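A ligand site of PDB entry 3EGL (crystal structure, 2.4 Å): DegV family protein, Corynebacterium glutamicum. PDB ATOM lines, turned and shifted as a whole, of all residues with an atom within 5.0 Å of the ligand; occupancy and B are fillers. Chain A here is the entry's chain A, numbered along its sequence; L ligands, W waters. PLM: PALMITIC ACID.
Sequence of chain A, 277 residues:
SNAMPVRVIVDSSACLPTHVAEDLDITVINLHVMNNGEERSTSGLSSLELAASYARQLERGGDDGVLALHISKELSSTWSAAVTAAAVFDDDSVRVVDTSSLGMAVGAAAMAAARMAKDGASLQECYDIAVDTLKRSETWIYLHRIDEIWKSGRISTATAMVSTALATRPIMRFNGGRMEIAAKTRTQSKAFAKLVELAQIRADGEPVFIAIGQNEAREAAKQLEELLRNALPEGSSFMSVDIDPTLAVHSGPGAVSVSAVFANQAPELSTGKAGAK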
ATOM      1  N   CYS A  15      35.637  14.308  21.129  1.00  0.00           N
ATOM      2  CA  CYS A  15      35.131  13.778  19.843  1.00  0.00           C
ATOM      3  C   CYS A  15      35.951  14.077  18.576  1.00  0.00           C
ATOM      4  O   CYS A  15      35.383  14.066  17.465  1.00  0.00           O
ATOM      5  CB  CYS A  15      33.679  14.215  19.591  1.00  0.00           C
ATOM      6  SG  CYS A  15      32.560  13.661  20.893  1.00  0.00           S
ATOM      7  N   LEU A  31      38.648   8.160  27.935  1.00  0.00           N
ATOM      8  CA  LEU A  31      37.849   7.903  29.158  1.00  0.00           C
ATOM      9  C   LEU A  31      37.474   6.403  29.218  1.00  0.00           C
ATOM     10  O   LEU A  31      37.656   5.688  28.239  1.00  0.00           O
ATOM     11  CB  LEU A  31      36.580   8.760  29.151  1.00  0.00           C
ATOM     12  CG  LEU A  31      36.833  10.259  29.006  1.00  0.00           C
ATOM     13  CD1 LEU A  31      35.512  11.098  28.809  1.00  0.00           C
ATOM     14  CD2 LEU A  31      37.642  10.696  30.220  1.00  0.00           C
ATOM     15  N   THR A  42      30.739   4.232  33.088  1.00  0.00           N
ATOM     16  CA  THR A  42      31.858   5.030  32.671  1.00  0.00           C
ATOM     17  C   THR A  42      32.615   5.602  33.849  1.00  0.00           C
ATOM     18  O   THR A  42      32.125   5.660  34.944  1.00  0.00           O
ATOM     19  CB  THR A  42      31.451   6.166  31.704  1.00  0.00           C
ATOM     20  OG1 THR A  42      30.814   7.238  32.426  1.00  0.00           O
ATOM     21  CG2 THR A  42      30.526   5.656  30.597  1.00  0.00           C
ATOM     22  N   SER A  43      33.803   6.078  33.569  1.00  0.00           N
ATOM     23  CA  SER A  43      34.700   6.508  34.589  1.00  0.00           C
ATOM     24  C   SER A  43      35.605   7.620  34.022  1.00  0.00           C
ATOM     25  O   SER A  43      36.071   7.548  32.876  1.00  0.00           O
ATOM     26  CB  SER A  43      35.514   5.282  34.940  1.00  0.00           C
ATOM     27  OG  SER A  43      36.399   5.580  35.952  1.00  0.00           O
ATOM     28  N   GLY A  44      35.830   8.652  34.810  1.00  0.00           N
ATOM     29  CA  GLY A  44      36.803   9.684  34.420  1.00  0.00           C
ATOM     30  C   GLY A  44      38.231   9.184  34.479  1.00  0.00           C
ATOM     31  O   GLY A  44      38.485   8.040  34.850  1.00  0.00           O
ATOM     32  N   ILE A  71      36.933  17.300  29.434  1.00  0.00           N
ATOM     33  CA  ILE A  71      35.554  17.363  29.849  1.00  0.00           C
ATOM     34  C   ILE A  71      35.322  18.195  31.153  1.00  0.00           C
ATOM     35  O   ILE A  71      36.114  18.146  32.139  1.00  0.00           O
ATOM     36  CB  ILE A  71      34.957  15.925  29.982  1.00  0.00           C
ATOM     37  CG1 ILE A  71      33.469  15.935  30.347  1.00  0.00           C
ATOM     38  CG2 ILE A  71      35.783  15.081  30.925  1.00  0.00           C
ATOM     39  CD1 ILE A  71      32.747  14.689  29.937  1.00  0.00           C
ATOM     40  N   LEU A  75      30.689  17.391  34.941  1.00  0.00           N
ATOM     41  CA  LEU A  75      30.143  16.216  34.306  1.00  0.00           C
ATOM     42  C   LEU A  75      31.022  15.038  34.659  1.00  0.00           C
ATOM     43  O   LEU A  75      30.612  13.879  34.522  1.00  0.00           O
ATOM     44  CB  LEU A  75      30.110  16.411  32.802  1.00  0.00           C
ATOM     45  CG  LEU A  75      29.202  17.555  32.358  1.00  0.00           C
ATOM     46  CD1 LEU A  75      29.202  17.713  30.859  1.00  0.00           C
ATOM     47  CD2 LEU A  75      27.708  17.449  32.873  1.00  0.00           C
ATOM     48  N   SER A  76      32.229  15.330  35.129  1.00  0.00           N
ATOM     49  CA  SER A  76      33.244  14.273  35.309  1.00  0.00           C
ATOM     50  C   SER A  76      34.275  14.641  36.378  1.00  0.00           C
ATOM     51  O   SER A  76      34.558  15.837  36.604  1.00  0.00           O
ATOM     52  CB  SER A  76      33.963  14.043  33.984  1.00  0.00           C
ATOM     53  OG  SER A  76      34.914  12.989  34.120  1.00  0.00           O
ATOM     54  N   SER A  77      34.859  13.634  37.006  1.00  0.00           N
ATOM     55  CA  SER A  77      35.948  13.842  37.971  1.00  0.00           C
ATOM     56  C   SER A  77      37.284  14.120  37.249  1.00  0.00           C
ATOM     57  O   SER A  77      38.302  14.335  37.878  1.00  0.00           O
ATOM     58  CB  SER A  77      36.086  12.605  38.846  1.00  0.00           C
ATOM     59  OG  SER A  77      36.438  11.445  38.080  1.00  0.00           O
ATOM     60  N   THR A  78      37.281  14.155  35.923  1.00  0.00           N
ATOM     61  CA  THR A  78      38.526  14.264  35.171  1.00  0.00           C
ATOM     62  C   THR A  78      39.341  15.514  35.452  1.00  0.00           C
ATOM     63  O   THR A  78      40.551  15.425  35.695  1.00  0.00           O
ATOM     64  CB  THR A  78      38.275  14.064  33.662  1.00  0.00           C
ATOM     65  OG1 THR A  78      37.833  12.720  33.476  1.00  0.00           O
ATOM     66  CG2 THR A  78      39.548  14.235  32.855  1.00  0.00           C
ATOM     67  N   LEU A 102      32.167  20.022  26.755  1.00  0.00           N
ATOM     68  CA  LEU A 102      32.541  18.709  26.309  1.00  0.00           C
ATOM     69  C   LEU A 102      32.317  18.655  24.798  1.00  0.00           C
ATOM     70  O   LEU A 102      31.645  19.539  24.219  1.00  0.00           O
ATOM     71  CB  LEU A 102      31.682  17.652  27.014  1.00  0.00           C
ATOM     72  CG  LEU A 102      30.219  17.509  26.572  1.00  0.00           C
ATOM     73  CD1 LEU A 102      29.566  16.364  27.325  1.00  0.00           C
ATOM     74  CD2 LEU A 102      29.415  18.796  26.733  1.00  0.00           C
ATOM     75  N   GLY A 103      32.857  17.622  24.160  1.00  0.00           N
ATOM     76  CA  GLY A 103      32.608  17.425  22.745  1.00  0.00           C
ATOM     77  C   GLY A 103      33.407  18.393  21.900  1.00  0.00           C
ATOM     78  O   GLY A 103      34.420  18.943  22.352  1.00  0.00           O
ATOM     79  N   THR A 139      26.926  24.280  22.918  1.00  0.00           N
ATOM     80  CA  THR A 139      26.763  22.834  22.717  1.00  0.00           C
ATOM     81  C   THR A 139      25.312  22.490  22.999  1.00  0.00           C
ATOM     82  O   THR A 139      24.815  22.681  24.129  1.00  0.00           O
ATOM     83  CB  THR A 139      27.755  22.022  23.633  1.00  0.00           C
ATOM     84  OG1 THR A 139      29.106  22.327  23.263  1.00  0.00           O
ATOM     85  CG2 THR A 139      27.547  20.506  23.524  1.00  0.00           C
ATOM     86  N   ILE A 141      22.356  19.216  22.435  1.00  0.00           N
ATOM     87  CA  ILE A 141      22.215  17.762  22.180  1.00  0.00           C
ATOM     88  C   ILE A 141      20.740  17.418  22.037  1.00  0.00           C
ATOM     89  O   ILE A 141      19.900  17.824  22.851  1.00  0.00           O
ATOM     90  CB  ILE A 141      22.774  16.878  23.338  1.00  0.00           C
ATOM     91  CG1 ILE A 141      24.093  17.418  23.851  1.00  0.00           C
ATOM     92  CG2 ILE A 141      22.995  15.377  22.890  1.00  0.00           C
ATOM     93  CD1 ILE A 141      24.426  16.853  25.235  1.00  0.00           C
ATOM     94  N   ILE A 149      20.334   9.422  29.404  1.00  0.00           N
ATOM     95  CA  ILE A 149      20.605  10.702  30.097  1.00  0.00           C
ATOM     96  C   ILE A 149      20.102  10.735  31.539  1.00  0.00           C
ATOM     97  O   ILE A 149      20.794  11.252  32.461  1.00  0.00           O
ATOM     98  CB  ILE A 149      20.093  11.952  29.364  1.00  0.00           C
ATOM     99  CG1 ILE A 149      20.901  13.160  29.828  1.00  0.00           C
ATOM    100  CG2 ILE A 149      18.611  12.225  29.627  1.00  0.00           C
ATOM    101  CD1 ILE A 149      22.190  13.275  29.123  1.00  0.00           C
ATOM    102  N   ARG A 154      23.631  13.224  35.542  1.00  0.00           N
ATOM    103  CA  ARG A 154      24.076  14.551  35.157  1.00  0.00           C
ATOM    104  C   ARG A 154      22.915  15.532  34.944  1.00  0.00           C
ATOM    105  O   ARG A 154      23.139  16.668  34.506  1.00  0.00           O
ATOM    106  CB  ARG A 154      24.932  14.473  33.884  1.00  0.00           C
ATOM    107  CG  ARG A 154      26.413  14.191  34.154  1.00  0.00           C
ATOM    108  CD  ARG A 154      26.646  12.730  34.471  1.00  0.00           C
ATOM    109  NE  ARG A 154      28.079  12.473  34.563  1.00  0.00           N
ATOM    110  CZ  ARG A 154      28.607  11.267  34.764  1.00  0.00           C
ATOM    111  NH1 ARG A 154      27.840  10.179  34.873  1.00  0.00           N
ATOM    112  NH2 ARG A 154      29.912  11.163  34.816  1.00  0.00           N
ATOM    113  N   PHE A 174      24.373  22.752  27.368  1.00  0.00           N
ATOM    114  CA  PHE A 174      25.294  23.078  28.472  1.00  0.00           C
ATOM    115  C   PHE A 174      25.495  24.532  28.704  1.00  0.00           C
ATOM    116  O   PHE A 174      25.924  25.213  27.815  1.00  0.00           O
ATOM    117  CB  PHE A 174      26.638  22.473  28.197  1.00  0.00           C
ATOM    118  CG  PHE A 174      26.564  21.028  28.151  1.00  0.00           C
ATOM    119  CD1 PHE A 174      26.672  20.288  29.305  1.00  0.00           C
ATOM    120  CD2 PHE A 174      26.248  20.400  26.935  1.00  0.00           C
ATOM    121  CE1 PHE A 174      26.530  18.875  29.266  1.00  0.00           C
ATOM    122  CE2 PHE A 174      26.111  18.995  26.852  1.00  0.00           C
ATOM    123  CZ  PHE A 174      26.258  18.216  28.040  1.00  0.00           C
ATOM    124  N   MET A 179      23.988  20.896  32.846  1.00  0.00           N
ATOM    125  CA  MET A 179      23.173  20.440  31.738  1.00  0.00           C
ATOM    126  C   MET A 179      21.708  20.899  31.830  1.00  0.00           C
ATOM    127  O   MET A 179      21.050  20.617  32.810  1.00  0.00           O
ATOM    128  CB  MET A 179      23.218  18.926  31.726  1.00  0.00           C
ATOM    129  CG  MET A 179      22.403  18.380  30.639  1.00  0.00           C
ATOM    130  SD  MET A 179      23.514  18.004  29.145  1.00  0.00           S
ATOM    131  CE  MET A 179      23.617  16.172  29.779  1.00  0.00           C
ATOM    132  N   ILE A 243      30.104  10.725  18.162  1.00  0.00           N
ATOM    133  CA  ILE A 243      30.059  10.923  19.584  1.00  0.00           C
ATOM    134  C   ILE A 243      30.897   9.828  20.278  1.00  0.00           C
ATOM    135  O   ILE A 243      30.734   8.637  20.020  1.00  0.00           O
ATOM    136  CB  ILE A 243      28.610  10.967  20.098  1.00  0.00           C
ATOM    137  CG1 ILE A 243      27.928  12.277  19.619  1.00  0.00           C
ATOM    138  CG2 ILE A 243      28.597  10.852  21.623  1.00  0.00           C
ATOM    139  CD1 ILE A 243      26.336  12.352  19.748  1.00  0.00           C
ATOM    140  N   THR A 246      32.119   6.740  25.167  1.00  0.00           N
ATOM    141  CA  THR A 246      31.939   6.999  26.591  1.00  0.00           C
ATOM    142  C   THR A 246      30.727   7.878  26.818  1.00  0.00           C
ATOM    143  O   THR A 246      29.969   7.659  27.774  1.00  0.00           O
ATOM    144  CB  THR A 246      33.168   7.652  27.230  1.00  0.00           C
ATOM    145  OG1 THR A 246      34.317   6.833  26.976  1.00  0.00           O
ATOM    146  CG2 THR A 246      33.014   7.751  28.751  1.00  0.00           C
ATOM    147  N   LEU A 247      30.555   8.882  25.948  1.00  0.00           N
ATOM    148  CA  LEU A 247      29.394   9.725  26.035  1.00  0.00           C
ATOM    149  C   LEU A 247      28.153   9.007  25.526  1.00  0.00           C
ATOM    150  O   LEU A 247      27.060   9.266  26.014  1.00  0.00           O
ATOM    151  CB  LEU A 247      29.621  11.052  25.300  1.00  0.00           C
ATOM    152  CG  LEU A 247      30.926  11.803  25.634  1.00  0.00           C
ATOM    153  CD1 LEU A 247      31.061  13.049  24.755  1.00  0.00           C
ATOM    154  CD2 LEU A 247      31.018  12.150  27.145  1.00  0.00           C
ATOM    155  N   HIS A 250      25.813   7.577  27.886  1.00  0.00           N
ATOM    156  CA  HIS A 250      24.898   8.437  28.598  1.00  0.00           C
ATOM    157  C   HIS A 250      23.930   9.197  27.725  1.00  0.00           C
ATOM    158  O   HIS A 250      22.929   9.716  28.222  1.00  0.00           O
ATOM    159  CB  HIS A 250      25.673   9.387  29.503  1.00  0.00           C
ATOM    160  CG  HIS A 250      26.540   8.695  30.511  1.00  0.00           C
ATOM    161  ND1 HIS A 250      26.023   7.881  31.509  1.00  0.00           N
ATOM    162  CD2 HIS A 250      27.886   8.706  30.702  1.00  0.00           C
ATOM    163  CE1 HIS A 250      27.024   7.421  32.252  1.00  0.00           C
ATOM    164  NE2 HIS A 250      28.161   7.894  31.764  1.00  0.00           N
ATOM    165  N   SER A 251      24.224   9.319  26.439  1.00  0.00           N
ATOM    166  CA  SER A 251      23.290   9.938  25.506  1.00  0.00           C
ATOM    167  C   SER A 251      22.263   8.937  24.966  1.00  0.00           C
ATOM    168  O   SER A 251      21.170   9.319  24.646  1.00  0.00           O
ATOM    169  CB  SER A 251      24.009  10.561  24.316  1.00  0.00           C
ATOM    170  OG  SER A 251      24.654   9.564  23.506  1.00  0.00           O
ATOM    171  N   SER A 257      24.428  15.685  18.383  1.00  0.00           N
ATOM    172  CA  SER A 257      24.942  16.891  19.037  1.00  0.00           C
ATOM    173  C   SER A 257      25.335  17.955  17.985  1.00  0.00           C
ATOM    174  O   SER A 257      25.764  17.636  16.862  1.00  0.00           O
ATOM    175  CB  SER A 257      26.159  16.538  19.931  1.00  0.00           C
ATOM    176  OG  SER A 257      27.268  16.040  19.164  1.00  0.00           O
ATOM    177  N   SER A 259      27.907  21.153  18.047  1.00  0.00           N
ATOM    178  CA  SER A 259      28.914  21.985  18.726  1.00  0.00           C
ATOM    179  C   SER A 259      29.201  23.117  17.778  1.00  0.00           C
ATOM    180  O   SER A 259      29.533  22.882  16.590  1.00  0.00           O
ATOM    181  CB  SER A 259      30.193  21.202  19.001  1.00  0.00           C
ATOM    182  OG  SER A 259      29.924  19.921  19.598  1.00  0.00           O
HETATM  183  C1  PLM L   1      32.935   9.955  33.381  1.00  0.00           C
HETATM  184  O1  PLM L   1      33.240  10.919  34.112  1.00  0.00           O
HETATM  185  O2  PLM L   1      32.385   8.973  33.918  1.00  0.00           O
HETATM  186  C2  PLM L   1      33.152   9.946  31.897  1.00  0.00           C
HETATM  187  C3  PLM L   1      32.286  11.048  31.278  1.00  0.00           C
HETATM  188  C4  PLM L   1      30.822  10.731  31.130  1.00  0.00           C
HETATM  189  C5  PLM L   1      30.132  12.091  30.959  1.00  0.00           C
HETATM  190  C6  PLM L   1      28.675  11.957  30.617  1.00  0.00           C
HETATM  191  C7  PLM L   1      28.082  13.345  30.514  1.00  0.00           C
HETATM  192  C8  PLM L   1      26.734  13.400  29.777  1.00  0.00           C
HETATM  193  C9  PLM L   1      26.944  13.245  28.267  1.00  0.00           C
HETATM  194  CA  PLM L   1      25.785  13.838  27.442  1.00  0.00           C
HETATM  195  CB  PLM L   1      25.726  13.289  26.023  1.00  0.00           C
HETATM  196  CC  PLM L   1      26.958  13.559  25.132  1.00  0.00           C
HETATM  197  CD  PLM L   1      26.795  14.850  24.358  1.00  0.00           C
HETATM  198  CE  PLM L   1      27.578  14.867  23.057  1.00  0.00           C
HETATM  199  CF  PLM L   1      28.727  15.865  23.115  1.00  0.00           C
HETATM  200  CG  PLM L   1      28.395  17.246  22.545  1.00  0.00           C
HETATM  201  O   HOH W   1      33.448  10.933  36.723  1.00  0.00           O
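An oxygen (O2) of the ligand lies within hydrogen-bond range of the side-chain hydroxyl (OG1) of Thr 42 (2.8 Å).
The guanidinium group (NH2) of Arg 154 is in salt-bridge range of an oxygen (O1) of the ligand (3.4 Å).
An oxygen (O1) of the ligand is in hydrogen-bond range of the side-chain hydroxyl (OG) of Ser 76.
N of Ser 43 lies within hydrogen-bond range of O2 of the ligand (3.2 Å).
Gly 44 touches the ligand.
Ile 71 touches the ligand.
Leu 75 touches the ligand (O to O1, 3.98 Å).
CG2 of Thr 139 touches CG of the ligand (3.5 Å).
Ile 141 touches the ligand (CD1 to CD, 3.2 Å).
Met 179 touches the ligand.
CG2 of Thr 246 touches C2 of the ligand (3.8 Å).
Leu 247 touches the ligand (CB to CC, 3.7 Å).
His 250 touches the ligand (CD2 to C6, 3.3 Å).
Ser 251 touches the ligand (CB to CB, 3.6 Å).
Ser 257 touches the ligand.
Hydrophobic or aromatic side chains that line the ligand: Ile 71, Ile 141, Met 179, Leu 247 and His 250.
15 residues have an atom within 4 Å of the ligand: Thr 42, Ser 43, Gly 44, Ile 71, Leu 75, Ser 76, Thr 139, Ile 141, Arg 154, Met 179, Thr 246, Leu 247, His 250, Ser 251 and Ser 257.
Along chain A the residues within 4 Å of the ligand span positions 42 to 257.
NH2 of Arg 154 sits at hydrogen-bond distance from O of Leu 75, at 2.8 Å.
OG of Ser 251 sits at hydrogen-bond distance from O of Leu 247 (3.5 Å).
The side-chain hydroxyl (OG) of Ser 76 is in hydrogen-bond range of the side-chain hydroxyl (OG1) of Thr 78 (3.0 Å).
A ring nitrogen (NE2) of His 250 lies within hydrogen-bond range of the side-chain hydroxyl of Thr 42.
N of Phe 174 sits at hydrogen-bond distance from O of Thr 139 (3.3 Å).
O of His 250 sits at hydrogen-bond distance from N of Ile 149 (2.9 Å).
Water W1 lies within hydrogen-bond range of O1 of the ligand (2.6 Å) and N of Ser 77 (3.1 Å).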
